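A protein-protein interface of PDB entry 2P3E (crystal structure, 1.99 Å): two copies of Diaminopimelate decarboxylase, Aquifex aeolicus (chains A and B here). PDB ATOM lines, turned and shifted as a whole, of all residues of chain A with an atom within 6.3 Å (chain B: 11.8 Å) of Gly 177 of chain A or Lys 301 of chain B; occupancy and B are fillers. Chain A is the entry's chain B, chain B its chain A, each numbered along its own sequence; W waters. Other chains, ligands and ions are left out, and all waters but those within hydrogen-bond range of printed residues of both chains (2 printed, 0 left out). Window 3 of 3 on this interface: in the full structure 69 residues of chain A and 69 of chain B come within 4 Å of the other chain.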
ATOM      1  N   VAL A 129      -3.921  17.842  14.361  1.00  0.00           N
ATOM      2  CA  VAL A 129      -3.790  19.039  15.143  1.00  0.00           C
ATOM      3  C   VAL A 129      -3.275  20.203  14.305  1.00  0.00           C
ATOM      4  O   VAL A 129      -2.314  20.072  13.528  1.00  0.00           O
ATOM      5  CB  VAL A 129      -2.919  18.798  16.423  1.00  0.00           C
ATOM      6  CG1 VAL A 129      -2.685  20.076  17.157  1.00  0.00           C
ATOM      7  CG2 VAL A 129      -3.617  17.809  17.371  1.00  0.00           C
ATOM      8  N   GLU A 130      -3.934  21.340  14.511  1.00  0.00           N
ATOM      9  CA  GLU A 130      -3.765  22.555  13.731  1.00  0.00           C
ATOM     10  C   GLU A 130      -3.002  23.669  14.462  1.00  0.00           C
ATOM     11  O   GLU A 130      -2.604  24.650  13.831  1.00  0.00           O
ATOM     12  CB  GLU A 130      -5.146  23.066  13.293  1.00  0.00           C
ATOM     13  CG  GLU A 130      -5.851  22.169  12.276  1.00  0.00           C
ATOM     14  CD  GLU A 130      -5.260  22.248  10.869  1.00  0.00           C
ATOM     15  OE1 GLU A 130      -4.356  23.083  10.615  1.00  0.00           O
ATOM     16  OE2 GLU A 130      -5.721  21.469  10.014  1.00  0.00           O
ATOM     17  N   ARG A 154      -0.691  18.386  11.663  1.00  0.00           N
ATOM     18  CA  ARG A 154      -0.904  18.737  10.269  1.00  0.00           C
ATOM     19  C   ARG A 154       0.280  19.534   9.740  1.00  0.00           C
ATOM     20  O   ARG A 154       0.538  20.648  10.205  1.00  0.00           O
ATOM     21  CB  ARG A 154      -2.181  19.541  10.034  1.00  0.00           C
ATOM     22  CG  ARG A 154      -2.391  19.697   8.518  1.00  0.00           C
ATOM     23  CD  ARG A 154      -3.502  20.631   8.185  1.00  0.00           C
ATOM     24  NE  ARG A 154      -3.650  20.842   6.737  1.00  0.00           N
ATOM     25  CZ  ARG A 154      -4.792  21.226   6.171  1.00  0.00           C
ATOM     26  NH1 ARG A 154      -5.871  21.427   6.923  1.00  0.00           N
ATOM     27  NH2 ARG A 154      -4.862  21.408   4.859  1.00  0.00           N
ATOM     28  N   VAL A 155       0.974  18.962   8.758  1.00  0.00           N
ATOM     29  CA  VAL A 155       2.163  19.584   8.187  1.00  0.00           C
ATOM     30  C   VAL A 155       1.895  20.077   6.775  1.00  0.00           C
ATOM     31  O   VAL A 155       1.139  19.439   6.028  1.00  0.00           O
ATOM     32  CB  VAL A 155       3.420  18.636   8.252  1.00  0.00           C
ATOM     33  CG1 VAL A 155       3.634  18.106   9.684  1.00  0.00           C
ATOM     34  CG2 VAL A 155       3.302  17.473   7.295  1.00  0.00           C
ATOM     35  N   ASN A 156       2.474  21.240   6.447  1.00  0.00           N
ATOM     36  CA  ASN A 156       2.427  21.826   5.114  1.00  0.00           C
ATOM     37  C   ASN A 156       3.758  21.556   4.413  1.00  0.00           C
ATOM     38  O   ASN A 156       4.755  22.216   4.702  1.00  0.00           O
ATOM     39  CB  ASN A 156       2.221  23.342   5.201  1.00  0.00           C
ATOM     40  CG  ASN A 156       0.927  23.724   5.874  1.00  0.00           C
ATOM     41  OD1 ASN A 156      -0.025  22.926   5.946  1.00  0.00           O
ATOM     42  ND2 ASN A 156       0.872  24.954   6.378  1.00  0.00           N
ATOM     43  N   SER A 174      -2.673  30.526   4.447  1.00  0.00           N
ATOM     44  CA  SER A 174      -3.914  29.977   5.004  1.00  0.00           C
ATOM     45  C   SER A 174      -3.764  29.742   6.495  1.00  0.00           C
ATOM     46  O   SER A 174      -2.648  29.734   7.014  1.00  0.00           O
ATOM     47  CB  SER A 174      -4.293  28.666   4.316  1.00  0.00           C
ATOM     48  OG  SER A 174      -3.809  27.536   5.030  1.00  0.00           O
ATOM     49  N   LYS A 175      -4.896  29.499   7.167  1.00  0.00           N
ATOM     50  CA  LYS A 175      -4.930  29.244   8.609  1.00  0.00           C
ATOM     51  C   LYS A 175      -4.498  27.819   8.965  1.00  0.00           C
ATOM     52  O   LYS A 175      -4.359  27.485  10.153  1.00  0.00           O
ATOM     53  CB  LYS A 175      -6.342  29.511   9.163  1.00  0.00           C
ATOM     54  CG  LYS A 175      -7.457  28.644   8.534  1.00  0.00           C
ATOM     55  CD  LYS A 175      -8.834  29.042   9.042  1.00  0.00           C
ATOM     56  CE  LYS A 175      -9.946  28.216   8.386  1.00  0.00           C
ATOM     57  NZ  LYS A 175     -11.307  28.752   8.699  1.00  0.00           N
ATOM     58  N   PHE A 176      -4.285  26.978   7.951  1.00  0.00           N
ATOM     59  CA  PHE A 176      -4.056  25.555   8.204  1.00  0.00           C
ATOM     60  C   PHE A 176      -2.582  25.120   8.255  1.00  0.00           C
ATOM     61  O   PHE A 176      -1.731  25.644   7.522  1.00  0.00           O
ATOM     62  CB  PHE A 176      -4.792  24.697   7.166  1.00  0.00           C
ATOM     63  CG  PHE A 176      -6.285  24.911   7.132  1.00  0.00           C
ATOM     64  CD1 PHE A 176      -7.096  24.440   8.162  1.00  0.00           C
ATOM     65  CD2 PHE A 176      -6.876  25.554   6.053  1.00  0.00           C
ATOM     66  CE1 PHE A 176      -8.473  24.624   8.131  1.00  0.00           C
ATOM     67  CE2 PHE A 176      -8.255  25.746   6.012  1.00  0.00           C
ATOM     68  CZ  PHE A 176      -9.054  25.269   7.054  1.00  0.00           C
ATOM     69  N   GLY A 177      -2.315  24.138   9.113  1.00  0.00           N
ATOM     70  CA  GLY A 177      -1.040  23.422   9.146  1.00  0.00           C
ATOM     71  C   GLY A 177       0.116  24.198   9.749  1.00  0.00           C
ATOM     72  O   GLY A 177      -0.033  25.347  10.203  1.00  0.00           O
ATOM     73  N   VAL A 178       1.270  23.551   9.778  1.00  0.00           N
ATOM     74  CA  VAL A 178       2.509  24.196  10.170  1.00  0.00           C
ATOM     75  C   VAL A 178       3.541  23.801   9.123  1.00  0.00           C
ATOM     76  O   VAL A 178       3.534  22.673   8.620  1.00  0.00           O
ATOM     77  CB  VAL A 178       2.950  23.815  11.625  1.00  0.00           C
ATOM     78  CG1 VAL A 178       3.272  22.319  11.768  1.00  0.00           C
ATOM     79  CG2 VAL A 178       4.139  24.642  12.082  1.00  0.00           C
ATOM     80  N   ASP A 179       4.406  24.748   8.779  1.00  0.00           N
ATOM     81  CA  ASP A 179       5.563  24.486   7.934  1.00  0.00           C
ATOM     82  C   ASP A 179       6.207  23.197   8.389  1.00  0.00           C
ATOM     83  O   ASP A 179       6.544  23.032   9.564  1.00  0.00           O
ATOM     84  CB  ASP A 179       6.570  25.642   8.053  1.00  0.00           C
ATOM     85  CG  ASP A 179       7.698  25.562   7.027  1.00  0.00           C
ATOM     86  OD1 ASP A 179       7.865  24.512   6.353  1.00  0.00           O
ATOM     87  OD2 ASP A 179       8.427  26.570   6.899  1.00  0.00           O
ATOM     88  N   GLU A 186       7.042  20.940  17.119  1.00  0.00           N
ATOM     89  CA  GLU A 186       5.745  20.616  17.694  1.00  0.00           C
ATOM     90  C   GLU A 186       5.638  19.174  18.175  1.00  0.00           C
ATOM     91  O   GLU A 186       4.950  18.914  19.151  1.00  0.00           O
ATOM     92  CB  GLU A 186       4.596  20.962  16.730  1.00  0.00           C
ATOM     93  CG  GLU A 186       4.195  22.433  16.797  1.00  0.00           C
ATOM     94  CD  GLU A 186       2.967  22.746  15.976  1.00  0.00           C
ATOM     95  OE1 GLU A 186       1.913  22.080  16.150  1.00  0.00           O
ATOM     96  OE2 GLU A 186       3.056  23.678  15.146  1.00  0.00           O
ATOM     97  N   PHE B 297      -8.618  29.677  19.573  1.00  0.00           N
ATOM     98  CA  PHE B 297      -7.167  29.485  19.506  1.00  0.00           C
ATOM     99  C   PHE B 297      -6.471  30.684  18.886  1.00  0.00           C
ATOM    100  O   PHE B 297      -7.055  31.396  18.067  1.00  0.00           O
ATOM    101  CB  PHE B 297      -6.802  28.247  18.686  1.00  0.00           C
ATOM    102  CG  PHE B 297      -7.493  26.988  19.127  1.00  0.00           C
ATOM    103  CD1 PHE B 297      -8.529  26.456  18.372  1.00  0.00           C
ATOM    104  CD2 PHE B 297      -7.089  26.323  20.275  1.00  0.00           C
ATOM    105  CE1 PHE B 297      -9.170  25.279  18.766  1.00  0.00           C
ATOM    106  CE2 PHE B 297      -7.718  25.148  20.676  1.00  0.00           C
ATOM    107  CZ  PHE B 297      -8.767  24.628  19.914  1.00  0.00           C
ATOM    108  N   LEU B 298      -5.227  30.901  19.303  1.00  0.00           N
ATOM    109  CA  LEU B 298      -4.326  31.804  18.609  1.00  0.00           C
ATOM    110  C   LEU B 298      -3.210  30.972  17.986  1.00  0.00           C
ATOM    111  O   LEU B 298      -2.710  30.036  18.619  1.00  0.00           O
ATOM    112  CB  LEU B 298      -3.715  32.827  19.580  1.00  0.00           C
ATOM    113  CG  LEU B 298      -4.597  33.671  20.508  1.00  0.00           C
ATOM    114  CD1 LEU B 298      -3.704  34.540  21.404  1.00  0.00           C
ATOM    115  CD2 LEU B 298      -5.563  34.545  19.724  1.00  0.00           C
ATOM    116  N   LYS B 299      -2.837  31.293  16.747  1.00  0.00           N
ATOM    117  CA  LYS B 299      -1.685  30.650  16.114  1.00  0.00           C
ATOM    118  C   LYS B 299      -0.932  31.603  15.192  1.00  0.00           C
ATOM    119  O   LYS B 299      -1.521  32.506  14.581  1.00  0.00           O
ATOM    120  CB  LYS B 299      -2.060  29.324  15.407  1.00  0.00           C
ATOM    121  CG  LYS B 299      -2.811  29.438  14.086  1.00  0.00           C
ATOM    122  CD  LYS B 299      -3.071  28.054  13.430  1.00  0.00           C
ATOM    123  CE  LYS B 299      -1.900  27.579  12.559  1.00  0.00           C
ATOM    124  NZ  LYS B 299      -2.236  26.349  11.754  1.00  0.00           N
ATOM    125  N   ASP B 300       0.383  31.396  15.122  1.00  0.00           N
ATOM    126  CA  ASP B 300       1.247  32.102  14.183  1.00  0.00           C
ATOM    127  C   ASP B 300       1.694  31.171  13.061  1.00  0.00           C
ATOM    128  O   ASP B 300       1.976  30.001  13.297  1.00  0.00           O
ATOM    129  CB  ASP B 300       2.498  32.636  14.902  1.00  0.00           C
ATOM    130  CG  ASP B 300       2.210  33.825  15.818  1.00  0.00           C
ATOM    131  OD1 ASP B 300       1.051  34.275  15.943  1.00  0.00           O
ATOM    132  OD2 ASP B 300       3.178  34.321  16.417  1.00  0.00           O
ATOM    133  N   LYS B 301       1.743  31.694  11.839  1.00  0.00           N
ATOM    134  CA  LYS B 301       2.428  31.026  10.736  1.00  0.00           C
ATOM    135  C   LYS B 301       3.414  32.022  10.154  1.00  0.00           C
ATOM    136  O   LYS B 301       3.015  33.005   9.525  1.00  0.00           O
ATOM    137  CB  LYS B 301       1.446  30.531   9.671  1.00  0.00           C
ATOM    138  CG  LYS B 301       0.847  29.167   9.992  1.00  0.00           C
ATOM    139  CD  LYS B 301      -0.200  28.739   8.979  1.00  0.00           C
ATOM    140  CE  LYS B 301       0.418  28.347   7.645  1.00  0.00           C
ATOM    141  NZ  LYS B 301      -0.623  27.945   6.687  1.00  0.00           N
ATOM    142  N   GLY B 302       4.701  31.774  10.382  1.00  0.00           N
ATOM    143  CA  GLY B 302       5.728  32.774  10.101  1.00  0.00           C
ATOM    144  C   GLY B 302       5.513  33.972  11.012  1.00  0.00           C
ATOM    145  O   GLY B 302       5.440  33.821  12.237  1.00  0.00           O
ATOM    146  N   SER B 303       5.372  35.146  10.400  1.00  0.00           N
ATOM    147  CA  SER B 303       5.115  36.411  11.094  1.00  0.00           C
ATOM    148  C   SER B 303       3.619  36.776  11.133  1.00  0.00           C
ATOM    149  O   SER B 303       3.222  37.754  11.773  1.00  0.00           O
ATOM    150  CB  SER B 303       5.895  37.528  10.402  1.00  0.00           C
ATOM    151  OG  SER B 303       5.669  37.491   8.999  1.00  0.00           O
ATOM    152  N   LYS B 304       2.805  35.994  10.425  1.00  0.00           N
ATOM    153  CA  LYS B 304       1.357  36.199  10.373  1.00  0.00           C
ATOM    154  C   LYS B 304       0.659  35.631  11.621  1.00  0.00           C
ATOM    155  O   LYS B 304       0.995  34.541  12.078  1.00  0.00           O
ATOM    156  CB  LYS B 304       0.803  35.541   9.107  1.00  0.00           C
ATOM    157  CG  LYS B 304      -0.575  36.012   8.718  1.00  0.00           C
ATOM    158  CD  LYS B 304      -0.930  35.518   7.340  1.00  0.00           C
ATOM    159  CE  LYS B 304      -2.332  35.964   6.975  1.00  0.00           C
ATOM    160  NZ  LYS B 304      -2.861  35.311   5.747  1.00  0.00           N
ATOM    161  N   HIS B 305      -0.315  36.374  12.150  1.00  0.00           N
ATOM    162  CA  HIS B 305      -1.075  35.970  13.332  1.00  0.00           C
ATOM    163  C   HIS B 305      -2.516  35.625  12.956  1.00  0.00           C
ATOM    164  O   HIS B 305      -3.144  36.332  12.170  1.00  0.00           O
ATOM    165  CB  HIS B 305      -1.064  37.084  14.392  1.00  0.00           C
ATOM    166  CG  HIS B 305       0.288  37.696  14.596  1.00  0.00           C
ATOM    167  ND1 HIS B 305       1.337  37.010  15.176  1.00  0.00           N
ATOM    168  CD2 HIS B 305       0.776  38.918  14.260  1.00  0.00           C
ATOM    169  CE1 HIS B 305       2.408  37.787  15.199  1.00  0.00           C
ATOM    170  NE2 HIS B 305       2.093  38.949  14.651  1.00  0.00           N
ATOM    171  N   PHE B 306      -3.019  34.539  13.529  1.00  0.00           N
ATOM    172  CA  PHE B 306      -4.399  34.117  13.319  1.00  0.00           C
ATOM    173  C   PHE B 306      -5.119  34.087  14.656  1.00  0.00           C
ATOM    174  O   PHE B 306      -4.589  33.596  15.647  1.00  0.00           O
ATOM    175  CB  PHE B 306      -4.444  32.728  12.685  1.00  0.00           C
ATOM    176  CG  PHE B 306      -3.837  32.667  11.316  1.00  0.00           C
ATOM    177  CD1 PHE B 306      -4.620  32.882  10.183  1.00  0.00           C
ATOM    178  CD2 PHE B 306      -2.485  32.393  11.155  1.00  0.00           C
ATOM    179  CE1 PHE B 306      -4.053  32.839   8.895  1.00  0.00           C
ATOM    180  CE2 PHE B 306      -1.910  32.338   9.874  1.00  0.00           C
ATOM    181  CZ  PHE B 306      -2.695  32.552   8.749  1.00  0.00           C
ATOM    182  N   ILE B 307      -6.330  34.628  14.670  1.00  0.00           N
ATOM    183  CA  ILE B 307      -7.232  34.500  15.807  1.00  0.00           C
ATOM    184  C   ILE B 307      -8.424  33.640  15.357  1.00  0.00           C
ATOM    185  O   ILE B 307      -9.237  34.055  14.530  1.00  0.00           O
ATOM    186  CB  ILE B 307      -7.707  35.881  16.313  1.00  0.00           C
ATOM    187  CG1 ILE B 307      -6.504  36.717  16.794  1.00  0.00           C
ATOM    188  CG2 ILE B 307      -8.799  35.727  17.413  1.00  0.00           C
ATOM    189  CD1 ILE B 307      -6.810  38.202  16.976  1.00  0.00           C
ATOM    190  N   ILE B 308      -8.501  32.445  15.915  1.00  0.00           N
ATOM    191  CA  ILE B 308      -9.505  31.471  15.515  1.00  0.00           C
ATOM    192  C   ILE B 308     -10.689  31.542  16.477  1.00  0.00           C
ATOM    193  O   ILE B 308     -10.524  31.382  17.688  1.00  0.00           O
ATOM    194  CB  ILE B 308      -8.894  30.043  15.465  1.00  0.00           C
ATOM    195  CG1 ILE B 308      -7.811  29.982  14.370  1.00  0.00           C
ATOM    196  CG2 ILE B 308      -9.983  28.991  15.233  1.00  0.00           C
ATOM    197  CD1 ILE B 308      -6.636  29.027  14.684  1.00  0.00           C
ATOM    198  N   VAL B 339      -2.243  44.253  17.774  1.00  0.00           N
ATOM    199  CA  VAL B 339      -1.814  43.179  16.881  1.00  0.00           C
ATOM    200  C   VAL B 339      -2.584  43.218  15.548  1.00  0.00           C
ATOM    201  O   VAL B 339      -3.761  43.588  15.516  1.00  0.00           O
ATOM    202  CB  VAL B 339      -1.937  41.777  17.575  1.00  0.00           C
ATOM    203  CG1 VAL B 339      -3.392  41.376  17.788  1.00  0.00           C
ATOM    204  CG2 VAL B 339      -1.209  40.693  16.787  1.00  0.00           C
ATOM    205  N   VAL B 340      -1.902  42.847  14.467  1.00  0.00           N
ATOM    206  CA  VAL B 340      -2.513  42.712  13.147  1.00  0.00           C
ATOM    207  C   VAL B 340      -2.738  41.213  12.892  1.00  0.00           C
ATOM    208  O   VAL B 340      -1.804  40.416  13.003  1.00  0.00           O
ATOM    209  CB  VAL B 340      -1.621  43.335  12.046  1.00  0.00           C
ATOM    210  CG1 VAL B 340      -2.172  43.024  10.638  1.00  0.00           C
ATOM    211  CG2 VAL B 340      -1.468  44.850  12.257  1.00  0.00           C
ATOM    212  N   ALA B 341      -3.973  40.827  12.578  1.00  0.00           N
ATOM    213  CA  ALA B 341      -4.313  39.402  12.473  1.00  0.00           C
ATOM    214  C   ALA B 341      -5.401  39.089  11.444  1.00  0.00           C
ATOM    215  O   ALA B 341      -6.203  39.960  11.094  1.00  0.00           O
ATOM    216  CB  ALA B 341      -4.720  38.848  13.850  1.00  0.00           C
ATOM    217  N   ASP B 342      -5.393  37.849  10.947  1.00  0.00           N
ATOM    218  CA  ASP B 342      -6.555  37.296  10.264  1.00  0.00           C
ATOM    219  C   ASP B 342      -7.480  36.765  11.370  1.00  0.00           C
ATOM    220  O   ASP B 342      -7.068  35.958  12.199  1.00  0.00           O
ATOM    221  CB  ASP B 342      -6.154  36.155   9.305  1.00  0.00           C
ATOM    222  CG  ASP B 342      -5.525  36.650   7.989  1.00  0.00           C
ATOM    223  OD1 ASP B 342      -5.234  37.864   7.827  1.00  0.00           O
ATOM    224  OD2 ASP B 342      -5.333  35.793   7.090  1.00  0.00           O
ATOM    225  N   VAL B 344     -10.381  34.375  11.850  1.00  0.00           N
ATOM    226  CA  VAL B 344     -10.900  33.292  11.016  1.00  0.00           C
ATOM    227  C   VAL B 344     -11.834  32.377  11.792  1.00  0.00           C
ATOM    228  O   VAL B 344     -11.747  32.299  13.006  1.00  0.00           O
ATOM    229  CB  VAL B 344      -9.742  32.468  10.383  1.00  0.00           C
ATOM    230  CG1 VAL B 344      -8.919  33.342   9.424  1.00  0.00           C
ATOM    231  CG2 VAL B 344      -8.851  31.831  11.470  1.00  0.00           C
ATOM    232  N   GLY B 345     -12.691  31.658  11.079  1.00  0.00           N
ATOM    233  CA  GLY B 345     -13.696  30.808  11.716  1.00  0.00           C
ATOM    234  C   GLY B 345     -13.328  29.342  11.798  1.00  0.00           C
ATOM    235  O   GLY B 345     -12.181  28.962  11.525  1.00  0.00           O
ATOM    236  N   PRO B 346     -14.309  28.497  12.170  1.00  0.00           N
ATOM    237  CA  PRO B 346     -14.127  27.055  12.307  1.00  0.00           C
ATOM    238  C   PRO B 346     -14.228  26.259  10.994  1.00  0.00           C
ATOM    239  O   PRO B 346     -13.798  25.102  10.945  1.00  0.00           O
ATOM    240  CB  PRO B 346     -15.288  26.663  13.235  1.00  0.00           C
ATOM    241  CG  PRO B 346     -16.376  27.625  12.892  1.00  0.00           C
ATOM    242  CD  PRO B 346     -15.680  28.917  12.526  1.00  0.00           C
ATOM    243  N   ILE B 347     -14.805  26.858   9.952  1.00  0.00           N
ATOM    244  CA  ILE B 347     -15.074  26.150   8.690  1.00  0.00           C
ATOM    245  C   ILE B 347     -13.775  25.697   8.001  1.00  0.00           C
ATOM    246  O   ILE B 347     -12.781  26.429   7.975  1.00  0.00           O
ATOM    247  CB  ILE B 347     -15.954  27.011   7.727  1.00  0.00           C
ATOM    248  CG1 ILE B 347     -17.355  27.262   8.325  1.00  0.00           C
ATOM    249  CG2 ILE B 347     -16.046  26.397   6.316  1.00  0.00           C
ATOM    250  CD1 ILE B 347     -18.158  25.986   8.620  1.00  0.00           C
ATOM    251  N   CYS B 348     -13.803  24.476   7.465  1.00  0.00           N
ATOM    252  CA  CYS B 348     -12.670  23.917   6.734  1.00  0.00           C
ATOM    253  C   CYS B 348     -12.585  24.490   5.315  1.00  0.00           C
ATOM    254  O   CYS B 348     -12.731  23.762   4.326  1.00  0.00           O
ATOM    255  CB  CYS B 348     -12.771  22.391   6.682  1.00  0.00           C
ATOM    256  SG  CYS B 348     -11.189  21.613   6.230  1.00  0.00           S
ATOM    257  N   GLU B 349     -12.396  25.804   5.227  1.00  0.00           N
ATOM    258  CA  GLU B 349     -12.141  26.498   3.961  1.00  0.00           C
ATOM    259  C   GLU B 349     -11.080  27.551   4.234  1.00  0.00           C
ATOM    260  O   GLU B 349     -11.145  28.246   5.248  1.00  0.00           O
ATOM    261  CB  GLU B 349     -13.402  27.202   3.448  1.00  0.00           C
ATOM    262  CG  GLU B 349     -14.477  26.307   2.876  1.00  0.00           C
ATOM    263  CD  GLU B 349     -14.204  25.869   1.431  1.00  0.00           C
ATOM    264  OE1 GLU B 349     -13.316  26.468   0.775  1.00  0.00           O
ATOM    265  OE2 GLU B 349     -14.891  24.932   0.950  1.00  0.00           O
ATOM    266  N   THR B 350     -10.118  27.682   3.325  1.00  0.00           N
ATOM    267  CA  THR B 350      -9.142  28.765   3.395  1.00  0.00           C
ATOM    268  C   THR B 350      -9.851  30.136   3.346  1.00  0.00           C
ATOM    269  O   THR B 350      -9.453  31.085   4.052  1.00  0.00           O
ATOM    270  CB  THR B 350      -8.092  28.627   2.258  1.00  0.00           C
ATOM    271  OG1 THR B 350      -7.386  27.391   2.438  1.00  0.00           O
ATOM    272  CG2 THR B 350      -7.091  29.778   2.301  1.00  0.00           C
ATOM    273  N   GLY B 351     -10.925  30.216   2.550  1.00  0.00           N
ATOM    274  CA  GLY B 351     -11.777  31.413   2.482  1.00  0.00           C
ATOM    275  C   GLY B 351     -12.701  31.676   3.675  1.00  0.00           C
ATOM    276  O   GLY B 351     -13.470  32.650   3.662  1.00  0.00           O
ATOM    277  N   ASP B 357      -5.910  40.707   7.884  1.00  0.00           N
ATOM    278  CA  ASP B 357      -4.913  41.745   8.169  1.00  0.00           C
ATOM    279  C   ASP B 357      -5.567  42.915   8.907  1.00  0.00           C
ATOM    280  O   ASP B 357      -5.493  44.077   8.473  1.00  0.00           O
ATOM    281  CB  ASP B 357      -4.202  42.207   6.874  1.00  0.00           C
ATOM    282  CG  ASP B 357      -3.417  41.080   6.198  1.00  0.00           C
ATOM    283  OD1 ASP B 357      -2.549  40.441   6.845  1.00  0.00           O
ATOM    284  OD2 ASP B 357      -3.664  40.837   5.001  1.00  0.00           O
HETATM  285  O   HOH W   1      -7.314  30.712   6.084  1.00  0.00           O
HETATM  286  O   HOH W   2      -7.810  22.101   5.238  1.00  0.00           O
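The side-chain amino group (NZ) of Lys 299 of chain B is in hydrogen-bond range of the backbone carbonyl oxygen (O) of Glu 130 of chain A (2.7 Å). O of Lys 175 of chain A is in hydrogen-bond range of NZ of Lys 299 of chain B (2.9 Å). NZ of Lys 299 of chain B is in hydrogen-bond range of O of Gly 177 of chain A (2.9 Å). The side-chain amide nitrogen of Asn 156 of chain A lies close to the side-chain amino group of Lys 301 of chain B (3.4 Å). O of Ser 174 of chain A lies within hydrogen-bond range of NZ of Lys 301 of chain B (2.7 Å). The side-chain amino group of Lys 301 of chain B is in hydrogen-bond range of the backbone carbonyl oxygen of Phe 176 of chain A (2.7 Å). The side-chain amino group of Lys 175 of chain A sits at hydrogen-bond distance from the backbone carbonyl oxygen of Gly 345 of chain B. The side-chain amino group (NZ) of Lys 175 of chain A is in hydrogen-bond range of the backbone carbonyl oxygen (O) of Ile 347 of chain B, 2.8 Å away. O of Glu 349 of chain B sits close to NZ of Lys 175 of chain A (3.5 Å).
The backbone carbonyl oxygen (O) of Lys 299 of chain B is in hydrogen-bond range of the backbone NH (N) of Phe 306 of chain B (2.7 Å). OE2 of Glu 130 of chain A lies within salt-bridge range of NH1 of Arg 154 of chain A, at 3.1 Å. The side-chain carboxylate of Glu 130 of chain A lies within hydrogen-bond range of the backbone NH of Gly 177 of chain A, 2.7 Å away. The side-chain amide nitrogen (ND2) of Asn 156 of chain A sits at hydrogen-bond distance from the backbone carbonyl oxygen (O) of Phe 176 of chain A (2.9 Å). The backbone NH (N) of Asn 156 of chain A sits at hydrogen-bond distance from the backbone carbonyl oxygen (O) of Val 178 of chain A (2.8 Å). The side-chain hydroxyl (OG) of Ser 174 of chain A sits at hydrogen-bond distance from the backbone NH (N) of Phe 176 of chain A (3.0 Å).
Ser 174 of chain A touches Phe 306 of chain B (O to CZ, 3.3 Å). Ser 174 of chain A touches Thr 350 of chain B (CB to CG2, 3.6 Å). CA of Lys 175 of chain A touches CE1 of Phe 306 of chain B (3.7 Å). Val 344 of chain B touches Lys 175 of chain A (CG2 to CD, 3.7 Å). Phe 176 of chain A touches Lys 299 of chain B (C to NZ, 3.7 Å). CZ of Phe 176 of chain A touches CA of Cys 348 of chain B, at 3.9 Å. Glu 349 of chain B touches Phe 176 of chain A. CE2 of Phe 176 of chain A touches N of Thr 350 of chain B, 3.8 Å away. Gly 177 of chain A touches Lys 301 of chain B (O to CD, 3.6 Å).
Printed residues of chain B within 4 Å of Gly 177 of chain A: Lys 299 and Lys 301. Of chain A, only Asn 156, Ser 174, Phe 176 and Gly 177 come within 4 Å of Lys 301 of chain B. Arg 154 of chain A touches none of the printed residues of chain B. Asn 156 of chain A touches just one residue of chain B: Lys 301. Of chain B, only Lys 301 (2.7 Å), Phe 306 (3.3 Å) and Thr 350 (3.6 Å) come within 4 Å of Ser 174 of chain A. Val 178 of chain A touches none of the printed residues of chain B. Printed residues of chain A within 4 Å of Cys 348 of chain B: Phe 176 (3.9 Å). Printed residues of chain A within 4 Å of Ile 347 of chain B: Lys 175. Printed residues of chain A within 4 Å of Phe 306 of chain B: Ser 174 (3.3 Å) and Lys 175 (3.7 Å). The nearest residue of chain B that does not touch Gly 177 of chain A is Asp 300 of chain B (5.9 Å). The nearest residue of chain A that does not touch Lys 301 of chain B is Lys 175 of chain A (4.4 Å). The nearest printed residue of chain A that does not touch Cys 348 of chain B is Lys 175 of chain A (5.1 Å).
Hydrophobic or aromatic side chains of chain A that line the printed part of chain B: Phe 176. Printed residues of chain B that touch a printed residue of chain A: Lys 299, Lys 301, Phe 306, Val 344, Gly 345, Ile 347, Cys 348, Glu 349 and Thr 350. Hydrophobic or aromatic side chains of chain B that line the printed part of chain A: Phe 306 and Val 344. Among the printed residues, 18 pairs touch across the chains. Among the printed residues, no Asp or Glu carboxylate lies within 4 Å of a Lys or Arg side-chain nitrogen of the other chain.
No position is printed for both chains. Of the 18 pairs that touch across the chains among the printed residues, none has its exchanged pair printed and touching as well.
Water W2 lies within hydrogen-bond range of the guanidinium group of Arg 154 of chain A and the side-chain sulfur of Cys 348 of chain B. Water W1 lies within hydrogen-bond range of N of Lys 175 of chain A and O of Thr 350 of chain B.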
